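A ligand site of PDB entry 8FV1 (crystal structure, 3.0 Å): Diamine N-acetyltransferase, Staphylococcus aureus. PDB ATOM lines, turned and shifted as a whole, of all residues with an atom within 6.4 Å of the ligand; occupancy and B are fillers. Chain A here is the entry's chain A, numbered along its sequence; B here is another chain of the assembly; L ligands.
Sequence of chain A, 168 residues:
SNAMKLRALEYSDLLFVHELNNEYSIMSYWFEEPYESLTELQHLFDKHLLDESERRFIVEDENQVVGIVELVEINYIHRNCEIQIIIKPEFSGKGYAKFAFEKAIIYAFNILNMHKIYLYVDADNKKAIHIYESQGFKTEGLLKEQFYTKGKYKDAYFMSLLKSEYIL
A nitrogen (N4) of the ligand is in salt-bridge range of the side-chain carboxylate of Glu 36 (3.7 Å).
OE1 of Glu 52 of chain B is in salt-bridge range of N2 of the ligand (3.3 Å).
A nitrogen (N3) of the ligand is in salt-bridge range of the side-chain carboxylate of Glu 32 (3.9 Å).
The side-chain carboxylate (OE1) of Glu 40 lies within salt-bridge range of a nitrogen (N2) of the ligand, 3.9 Å away.
N1 of the ligand sits close to O of His 48 of chain B.
OH of Tyr 107 of chain B is in hydrogen-bond range of OE2 of Glu 33 (2.6 Å).
The side-chain amide nitrogen of Asn 21 is in hydrogen-bond range of the side-chain carboxylate of Glu 36 (2.6 Å).
The side-chain hydroxyl (OH) of Tyr 35 lies within hydrogen-bond range of the backbone carbonyl oxygen (O) of Arg 56 of chain B (2.8 Å).
The side-chain amide oxygen (OD1) of Asn 21 sits close to the side-chain sulfur (SD) of Met 27 (3.8 Å).
The backbone carbonyl oxygen of Glu 36 lies within hydrogen-bond range of the side-chain amide nitrogen of Asn 22, at 3.1 Å.
The backbone NH (N) of Glu 32 is in hydrogen-bond range of the backbone carbonyl oxygen (O) of Met 27, at 2.9 Å.
The guanidinium group (NH1) of Arg 56 of chain B is in salt-bridge range of the side-chain carboxylate (OE1) of Glu 54 of chain B.
The side-chain carboxylate (OE1) of Glu 52 of chain B lies within salt-bridge range of the guanidinium group (NH2) of Arg 55 of chain B (3.2 Å).
Asn 21 touches the ligand (CB to C10, 3.9 Å).
Glu 33 touches the ligand (O to C9, 3.0 Å).
Tyr 35 touches the ligand (O to C5, 3.2 Å).
Leu 49 of chain B touches the ligand (O to C1, 3.0 Å).
Asp 51 of chain B touches the ligand.
Glu 54 of chain B touches the ligand (O to C2, 3.2 Å).
Arg 55 of chain B touches the ligand.
Hydrophobic or aromatic side chains within 4 Å of the ligand: Tyr 35.
Within 4 Å of the ligand: Asn 21, Glu 32, Glu 33, Tyr 35, Glu 36, Glu 40, His 48 of chain B, Leu 49 of chain B, Asp 51 of chain B, Glu 52 of chain B, Glu 54 of chain B and Arg 55 of chain B.
The nearest printed residue that does not touch the ligand is Met 27 (4.2 Å).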
ATOM      1  N   ASN A  21      20.426 -10.602   8.418  1.00  0.00           N
ATOM      2  CA  ASN A  21      19.944 -10.700   7.048  1.00  0.00           C
ATOM      3  C   ASN A  21      20.117  -9.414   6.252  1.00  0.00           C
ATOM      4  O   ASN A  21      19.747  -9.374   5.080  1.00  0.00           O
ATOM      5  CB  ASN A  21      18.463 -11.104   7.040  1.00  0.00           C
ATOM      6  CG  ASN A  21      18.260 -12.549   7.446  1.00  0.00           C
ATOM      7  OD1 ASN A  21      19.191 -13.356   7.409  1.00  0.00           O
ATOM      8  ND2 ASN A  21      17.031 -12.893   7.825  1.00  0.00           N
ATOM      9  N   ASN A  22      20.675  -8.356   6.863  1.00  0.00           N
ATOM     10  CA  ASN A  22      20.913  -7.103   6.176  1.00  0.00           C
ATOM     11  C   ASN A  22      22.394  -6.759   6.070  1.00  0.00           C
ATOM     12  O   ASN A  22      22.736  -5.640   5.683  1.00  0.00           O
ATOM     13  CB  ASN A  22      20.153  -5.957   6.864  1.00  0.00           C
ATOM     14  CG  ASN A  22      18.674  -5.987   6.566  1.00  0.00           C
ATOM     15  OD1 ASN A  22      18.201  -5.367   5.616  1.00  0.00           O
ATOM     16  ND2 ASN A  22      17.912  -6.706   7.386  1.00  0.00           N
ATOM     17  N   MET A  27      25.401 -12.199   4.008  1.00  0.00           N
ATOM     18  CA  MET A  27      24.463 -12.797   3.074  1.00  0.00           C
ATOM     19  C   MET A  27      25.142 -13.222   1.771  1.00  0.00           C
ATOM     20  O   MET A  27      24.636 -14.115   1.089  1.00  0.00           O
ATOM     21  CB  MET A  27      23.328 -11.823   2.775  1.00  0.00           C
ATOM     22  CG  MET A  27      22.358 -11.619   3.932  1.00  0.00           C
ATOM     23  SD  MET A  27      21.424 -13.102   4.353  1.00  0.00           S
ATOM     24  CE  MET A  27      22.366 -13.741   5.737  1.00  0.00           C
ATOM     25  N   TRP A  30      25.932 -16.790   1.726  1.00  0.00           N
ATOM     26  CA  TRP A  30      24.701 -17.536   1.491  1.00  0.00           C
ATOM     27  C   TRP A  30      24.133 -17.325   0.095  1.00  0.00           C
ATOM     28  O   TRP A  30      23.156 -17.989  -0.258  1.00  0.00           O
ATOM     29  CB  TRP A  30      23.636 -17.132   2.520  1.00  0.00           C
ATOM     30  CG  TRP A  30      23.701 -17.898   3.801  1.00  0.00           C
ATOM     31  CD1 TRP A  30      24.793 -18.498   4.349  1.00  0.00           C
ATOM     32  CD2 TRP A  30      22.602 -18.170   4.690  1.00  0.00           C
ATOM     33  NE1 TRP A  30      24.458 -19.118   5.529  1.00  0.00           N
ATOM     34  CE2 TRP A  30      23.121 -18.933   5.762  1.00  0.00           C
ATOM     35  CE3 TRP A  30      21.248 -17.839   4.692  1.00  0.00           C
ATOM     36  CZ2 TRP A  30      22.318 -19.364   6.818  1.00  0.00           C
ATOM     37  CZ3 TRP A  30      20.457 -18.273   5.743  1.00  0.00           C
ATOM     38  CH2 TRP A  30      20.991 -19.029   6.788  1.00  0.00           C
ATOM     39  N   GLU A  32      22.473 -14.879  -0.731  1.00  0.00           N
ATOM     40  CA  GLU A  32      21.193 -14.230  -0.522  1.00  0.00           C
ATOM     41  C   GLU A  32      21.327 -12.727  -0.766  1.00  0.00           C
ATOM     42  O   GLU A  32      22.405 -12.202  -1.067  1.00  0.00           O
ATOM     43  CB  GLU A  32      20.678 -14.507   0.883  1.00  0.00           C
ATOM     44  CG  GLU A  32      20.173 -15.917   1.099  1.00  0.00           C
ATOM     45  CD  GLU A  32      18.706 -16.086   0.755  1.00  0.00           C
ATOM     46  OE1 GLU A  32      18.155 -15.207   0.050  1.00  0.00           O
ATOM     47  OE2 GLU A  32      18.099 -17.083   1.200  1.00  0.00           O
ATOM     48  N   GLU A  33      20.200 -12.008  -0.641  1.00  0.00           N
ATOM     49  CA  GLU A  33      20.174 -10.552  -0.796  1.00  0.00           C
ATOM     50  C   GLU A  33      20.162  -9.894   0.563  1.00  0.00           C
ATOM     51  O   GLU A  33      19.389 -10.308   1.444  1.00  0.00           O
ATOM     52  CB  GLU A  33      18.947 -10.123  -1.592  1.00  0.00           C
ATOM     53  CG  GLU A  33      18.893  -8.643  -1.915  1.00  0.00           C
ATOM     54  CD  GLU A  33      17.745  -8.277  -2.824  1.00  0.00           C
ATOM     55  OE1 GLU A  33      17.078  -9.199  -3.354  1.00  0.00           O
ATOM     56  OE2 GLU A  33      17.497  -7.066  -3.016  1.00  0.00           O
ATOM     57  N   PRO A  34      20.988  -8.866   0.801  1.00  0.00           N
ATOM     58  CA  PRO A  34      21.019  -8.252   2.140  1.00  0.00           C
ATOM     59  C   PRO A  34      19.941  -7.194   2.316  1.00  0.00           C
ATOM     60  O   PRO A  34      20.209  -6.108   2.853  1.00  0.00           O
ATOM     61  CB  PRO A  34      22.426  -7.639   2.202  1.00  0.00           C
ATOM     62  CG  PRO A  34      22.708  -7.248   0.783  1.00  0.00           C
ATOM     63  CD  PRO A  34      21.998  -8.273  -0.095  1.00  0.00           C
ATOM     64  N   TYR A  35      18.718  -7.498   1.873  1.00  0.00           N
ATOM     65  CA  TYR A  35      17.591  -6.579   1.988  1.00  0.00           C
ATOM     66  C   TYR A  35      16.391  -7.365   2.493  1.00  0.00           C
ATOM     67  O   TYR A  35      15.844  -8.203   1.765  1.00  0.00           O
ATOM     68  CB  TYR A  35      17.282  -5.926   0.635  1.00  0.00           C
ATOM     69  CG  TYR A  35      16.189  -4.870   0.695  1.00  0.00           C
ATOM     70  CD1 TYR A  35      14.848  -5.233   0.711  1.00  0.00           C
ATOM     71  CD2 TYR A  35      16.508  -3.525   0.734  1.00  0.00           C
ATOM     72  CE1 TYR A  35      13.854  -4.281   0.760  1.00  0.00           C
ATOM     73  CE2 TYR A  35      15.513  -2.562   0.792  1.00  0.00           C
ATOM     74  CZ  TYR A  35      14.190  -2.941   0.807  1.00  0.00           C
ATOM     75  OH  TYR A  35      13.205  -1.992   0.860  1.00  0.00           O
ATOM     76  N   GLU A  36      15.985  -7.107   3.736  1.00  0.00           N
ATOM     77  CA  GLU A  36      14.829  -7.793   4.315  1.00  0.00           C
ATOM     78  C   GLU A  36      14.360  -6.969   5.513  1.00  0.00           C
ATOM     79  O   GLU A  36      14.977  -7.030   6.586  1.00  0.00           O
ATOM     80  CB  GLU A  36      15.185  -9.220   4.719  1.00  0.00           C
ATOM     81  CG  GLU A  36      13.984 -10.056   5.120  1.00  0.00           C
ATOM     82  CD  GLU A  36      14.362 -11.478   5.479  1.00  0.00           C
ATOM     83  OE1 GLU A  36      15.435 -11.677   6.096  1.00  0.00           O
ATOM     84  OE2 GLU A  36      13.590 -12.405   5.144  1.00  0.00           O
ATOM     85  N   GLU A  40       8.995  -7.827   6.795  1.00  0.00           N
ATOM     86  CA  GLU A  40       9.034  -8.987   5.895  1.00  0.00           C
ATOM     87  C   GLU A  40       9.543 -10.219   6.619  1.00  0.00           C
ATOM     88  O   GLU A  40       9.037 -11.324   6.408  1.00  0.00           O
ATOM     89  CB  GLU A  40       9.908  -8.668   4.685  1.00  0.00           C
ATOM     90  CG  GLU A  40      10.086  -9.838   3.726  1.00  0.00           C
ATOM     91  CD  GLU A  40      10.978  -9.494   2.543  1.00  0.00           C
ATOM     92  OE1 GLU A  40      11.276  -8.304   2.348  1.00  0.00           O
ATOM     93  OE2 GLU A  40      11.380 -10.424   1.809  1.00  0.00           O
ATOM     94  N   LEU A  44       7.452 -13.670   7.065  1.00  0.00           N
ATOM     95  CA  LEU A  44       7.947 -14.972   6.641  1.00  0.00           C
ATOM     96  C   LEU A  44       7.974 -15.953   7.808  1.00  0.00           C
ATOM     97  O   LEU A  44       7.630 -17.130   7.642  1.00  0.00           O
ATOM     98  CB  LEU A  44       9.340 -14.839   6.014  1.00  0.00           C
ATOM     99  CG  LEU A  44       9.410 -14.041   4.712  1.00  0.00           C
ATOM    100  CD1 LEU A  44      10.858 -13.918   4.253  1.00  0.00           C
ATOM    101  CD2 LEU A  44       8.564 -14.683   3.625  1.00  0.00           C
ATOM    102  N   HIS B  48       3.226  -3.099  -0.597  1.00  0.00           N
ATOM    103  CA  HIS B  48       4.389  -3.476  -1.400  1.00  0.00           C
ATOM    104  C   HIS B  48       5.497  -4.100  -0.558  1.00  0.00           C
ATOM    105  O   HIS B  48       6.662  -4.069  -0.966  1.00  0.00           O
ATOM    106  CB  HIS B  48       4.924  -2.239  -2.143  1.00  0.00           C
ATOM    107  CG  HIS B  48       3.902  -1.548  -2.977  1.00  0.00           C
ATOM    108  ND1 HIS B  48       3.617  -1.928  -4.275  1.00  0.00           N
ATOM    109  CD2 HIS B  48       3.088  -0.499  -2.707  1.00  0.00           C
ATOM    110  CE1 HIS B  48       2.673  -1.144  -4.767  1.00  0.00           C
ATOM    111  NE2 HIS B  48       2.333  -0.269  -3.836  1.00  0.00           N
ATOM    112  N   LEU B  49       5.155  -4.674   0.592  1.00  0.00           N
ATOM    113  CA  LEU B  49       6.170  -5.311   1.428  1.00  0.00           C
ATOM    114  C   LEU B  49       6.938  -6.373   0.658  1.00  0.00           C
ATOM    115  O   LEU B  49       8.169  -6.428   0.715  1.00  0.00           O
ATOM    116  CB  LEU B  49       5.511  -5.926   2.664  1.00  0.00           C
ATOM    117  CG  LEU B  49       6.451  -6.576   3.677  1.00  0.00           C
ATOM    118  CD1 LEU B  49       7.260  -5.526   4.408  1.00  0.00           C
ATOM    119  CD2 LEU B  49       5.671  -7.441   4.657  1.00  0.00           C
ATOM    120  N   LEU B  50       6.216  -7.210  -0.091  1.00  0.00           N
ATOM    121  CA  LEU B  50       6.825  -8.287  -0.852  1.00  0.00           C
ATOM    122  C   LEU B  50       6.907  -7.990  -2.348  1.00  0.00           C
ATOM    123  O   LEU B  50       7.220  -8.881  -3.136  1.00  0.00           O
ATOM    124  CB  LEU B  50       6.052  -9.594  -0.632  1.00  0.00           C
ATOM    125  CG  LEU B  50       5.802  -9.964   0.832  1.00  0.00           C
ATOM    126  CD1 LEU B  50       5.166 -11.341   0.933  1.00  0.00           C
ATOM    127  CD2 LEU B  50       7.100  -9.913   1.630  1.00  0.00           C
ATOM    128  N   ASP B  51       6.629  -6.753  -2.753  1.00  0.00           N
ATOM    129  CA  ASP B  51       6.755  -6.357  -4.153  1.00  0.00           C
ATOM    130  C   ASP B  51       8.229  -6.359  -4.533  1.00  0.00           C
ATOM    131  O   ASP B  51       8.989  -5.484  -4.110  1.00  0.00           O
ATOM    132  CB  ASP B  51       6.133  -4.988  -4.371  1.00  0.00           C
ATOM    133  CG  ASP B  51       6.158  -4.560  -5.829  1.00  0.00           C
ATOM    134  OD1 ASP B  51       6.571  -5.375  -6.681  1.00  0.00           O
ATOM    135  OD2 ASP B  51       5.763  -3.416  -6.122  1.00  0.00           O
ATOM    136  N   GLU B  52       8.647  -7.335  -5.332  1.00  0.00           N
ATOM    137  CA  GLU B  52      10.048  -7.472  -5.718  1.00  0.00           C
ATOM    138  C   GLU B  52      10.473  -6.455  -6.770  1.00  0.00           C
ATOM    139  O   GLU B  52      11.671  -6.365  -7.060  1.00  0.00           O
ATOM    140  CB  GLU B  52      10.312  -8.889  -6.219  1.00  0.00           C
ATOM    141  CG  GLU B  52      10.027  -9.980  -5.198  1.00  0.00           C
ATOM    142  CD  GLU B  52      10.886  -9.858  -3.952  1.00  0.00           C
ATOM    143  OE1 GLU B  52      11.876  -9.094  -3.976  1.00  0.00           O
ATOM    144  OE2 GLU B  52      10.568 -10.530  -2.945  1.00  0.00           O
ATOM    145  N   SER B  53       9.538  -5.702  -7.353  1.00  0.00           N
ATOM    146  CA  SER B  53       9.875  -4.640  -8.284  1.00  0.00           C
ATOM    147  C   SER B  53      10.300  -3.356  -7.579  1.00  0.00           C
ATOM    148  O   SER B  53      10.478  -2.336  -8.246  1.00  0.00           O
ATOM    149  CB  SER B  53       8.683  -4.355  -9.203  1.00  0.00           C
ATOM    150  OG  SER B  53       7.573  -3.888  -8.474  1.00  0.00           O
ATOM    151  N   GLU B  54      10.452  -3.386  -6.251  1.00  0.00           N
ATOM    152  CA  GLU B  54      10.803  -2.217  -5.467  1.00  0.00           C
ATOM    153  C   GLU B  54      11.949  -2.562  -4.540  1.00  0.00           C
ATOM    154  O   GLU B  54      12.025  -3.666  -4.007  1.00  0.00           O
ATOM    155  CB  GLU B  54       9.607  -1.726  -4.636  1.00  0.00           C
ATOM    156  CG  GLU B  54       8.283  -1.624  -5.396  1.00  0.00           C
ATOM    157  CD  GLU B  54       8.206  -0.404  -6.293  1.00  0.00           C
ATOM    158  OE1 GLU B  54       9.101   0.460  -6.216  1.00  0.00           O
ATOM    159  OE2 GLU B  54       7.232  -0.315  -7.074  1.00  0.00           O
ATOM    160  N   ARG B  55      12.852  -1.599  -4.339  1.00  0.00           N
ATOM    161  CA  ARG B  55      13.923  -1.692  -3.350  1.00  0.00           C
ATOM    162  C   ARG B  55      14.124  -0.294  -2.777  1.00  0.00           C
ATOM    163  O   ARG B  55      14.773   0.550  -3.417  1.00  0.00           O
ATOM    164  CB  ARG B  55      15.212  -2.239  -3.949  1.00  0.00           C
ATOM    165  CG  ARG B  55      15.144  -3.692  -4.405  1.00  0.00           C
ATOM    166  CD  ARG B  55      14.950  -4.647  -3.238  1.00  0.00           C
ATOM    167  NE  ARG B  55      15.233  -6.021  -3.626  1.00  0.00           N
ATOM    168  CZ  ARG B  55      14.410  -6.796  -4.338  1.00  0.00           C
ATOM    169  NH1 ARG B  55      13.246  -6.344  -4.759  1.00  0.00           N
ATOM    170  NH2 ARG B  55      14.782  -8.032  -4.626  1.00  0.00           N
ATOM    171  N   ARG B  56      13.556  -0.036  -1.605  1.00  0.00           N
ATOM    172  CA  ARG B  56      13.578   1.291  -0.992  1.00  0.00           C
ATOM    173  C   ARG B  56      14.568   1.292   0.160  1.00  0.00           C
ATOM    174  O   ARG B  56      14.463   0.483   1.087  1.00  0.00           O
ATOM    175  CB  ARG B  56      12.178   1.676  -0.511  1.00  0.00           C
ATOM    176  CG  ARG B  56      11.165   1.766  -1.650  1.00  0.00           C
ATOM    177  CD  ARG B  56       9.820   2.303  -1.184  1.00  0.00           C
ATOM    178  NE  ARG B  56       9.085   2.903  -2.299  1.00  0.00           N
ATOM    179  CZ  ARG B  56       8.377   2.223  -3.191  1.00  0.00           C
ATOM    180  NH1 ARG B  56       8.272   0.904  -3.129  1.00  0.00           N
ATOM    181  NH2 ARG B  56       7.755   2.879  -4.165  1.00  0.00           N
ATOM    182  N   TYR B 107      24.495  -1.493  -5.679  1.00  0.00           N
ATOM    183  CA  TYR B 107      23.482  -2.489  -5.345  1.00  0.00           C
ATOM    184  C   TYR B 107      22.753  -2.964  -6.595  1.00  0.00           C
ATOM    185  O   TYR B 107      22.474  -4.162  -6.742  1.00  0.00           O
ATOM    186  CB  TYR B 107      22.485  -1.906  -4.338  1.00  0.00           C
ATOM    187  CG  TYR B 107      21.635  -2.941  -3.644  1.00  0.00           C
ATOM    188  CD1 TYR B 107      20.629  -3.619  -4.314  1.00  0.00           C
ATOM    189  CD2 TYR B 107      21.842  -3.249  -2.306  1.00  0.00           C
ATOM    190  CE1 TYR B 107      19.849  -4.568  -3.686  1.00  0.00           C
ATOM    191  CE2 TYR B 107      21.079  -4.193  -1.660  1.00  0.00           C
ATOM    192  CZ  TYR B 107      20.077  -4.851  -2.352  1.00  0.00           C
ATOM    193  OH  TYR B 107      19.305  -5.793  -1.711  1.00  0.00           O
HETATM  194  N1  LIG L   1       9.703  -3.244  -1.378  1.00  0.00           N
HETATM  195  C1  LIG L   1       9.650  -4.687  -1.193  1.00  0.00           C
HETATM  196  C2  LIG L   1      11.041  -5.264  -1.416  1.00  0.00           C
HETATM  197  C3  LIG L   1      11.060  -6.735  -1.011  1.00  0.00           C
HETATM  198  N2  LIG L   1      12.389  -7.284  -1.231  1.00  0.00           N
HETATM  199  C4  LIG L   1      12.490  -8.607  -0.630  1.00  0.00           C
HETATM  200  C5  LIG L   1      13.946  -9.073  -0.695  1.00  0.00           C
HETATM  201  C6  LIG L   1      14.089 -10.402   0.034  1.00  0.00           C
HETATM  202  C7  LIG L   1      15.528 -10.913  -0.099  1.00  0.00           C
HETATM  203  N3  LIG L   1      15.587 -12.322   0.263  1.00  0.00           N
HETATM  204  C8  LIG L   1      15.673 -12.460   1.706  1.00  0.00           C
HETATM  205  C9  LIG L   1      17.097 -12.146   2.168  1.00  0.00           C
HETATM  206  C10 LIG L   1      17.284 -12.598   3.623  1.00  0.00           C
HETATM  207  N4  LIG L   1      17.004 -14.021   3.718  1.00  0.00           N
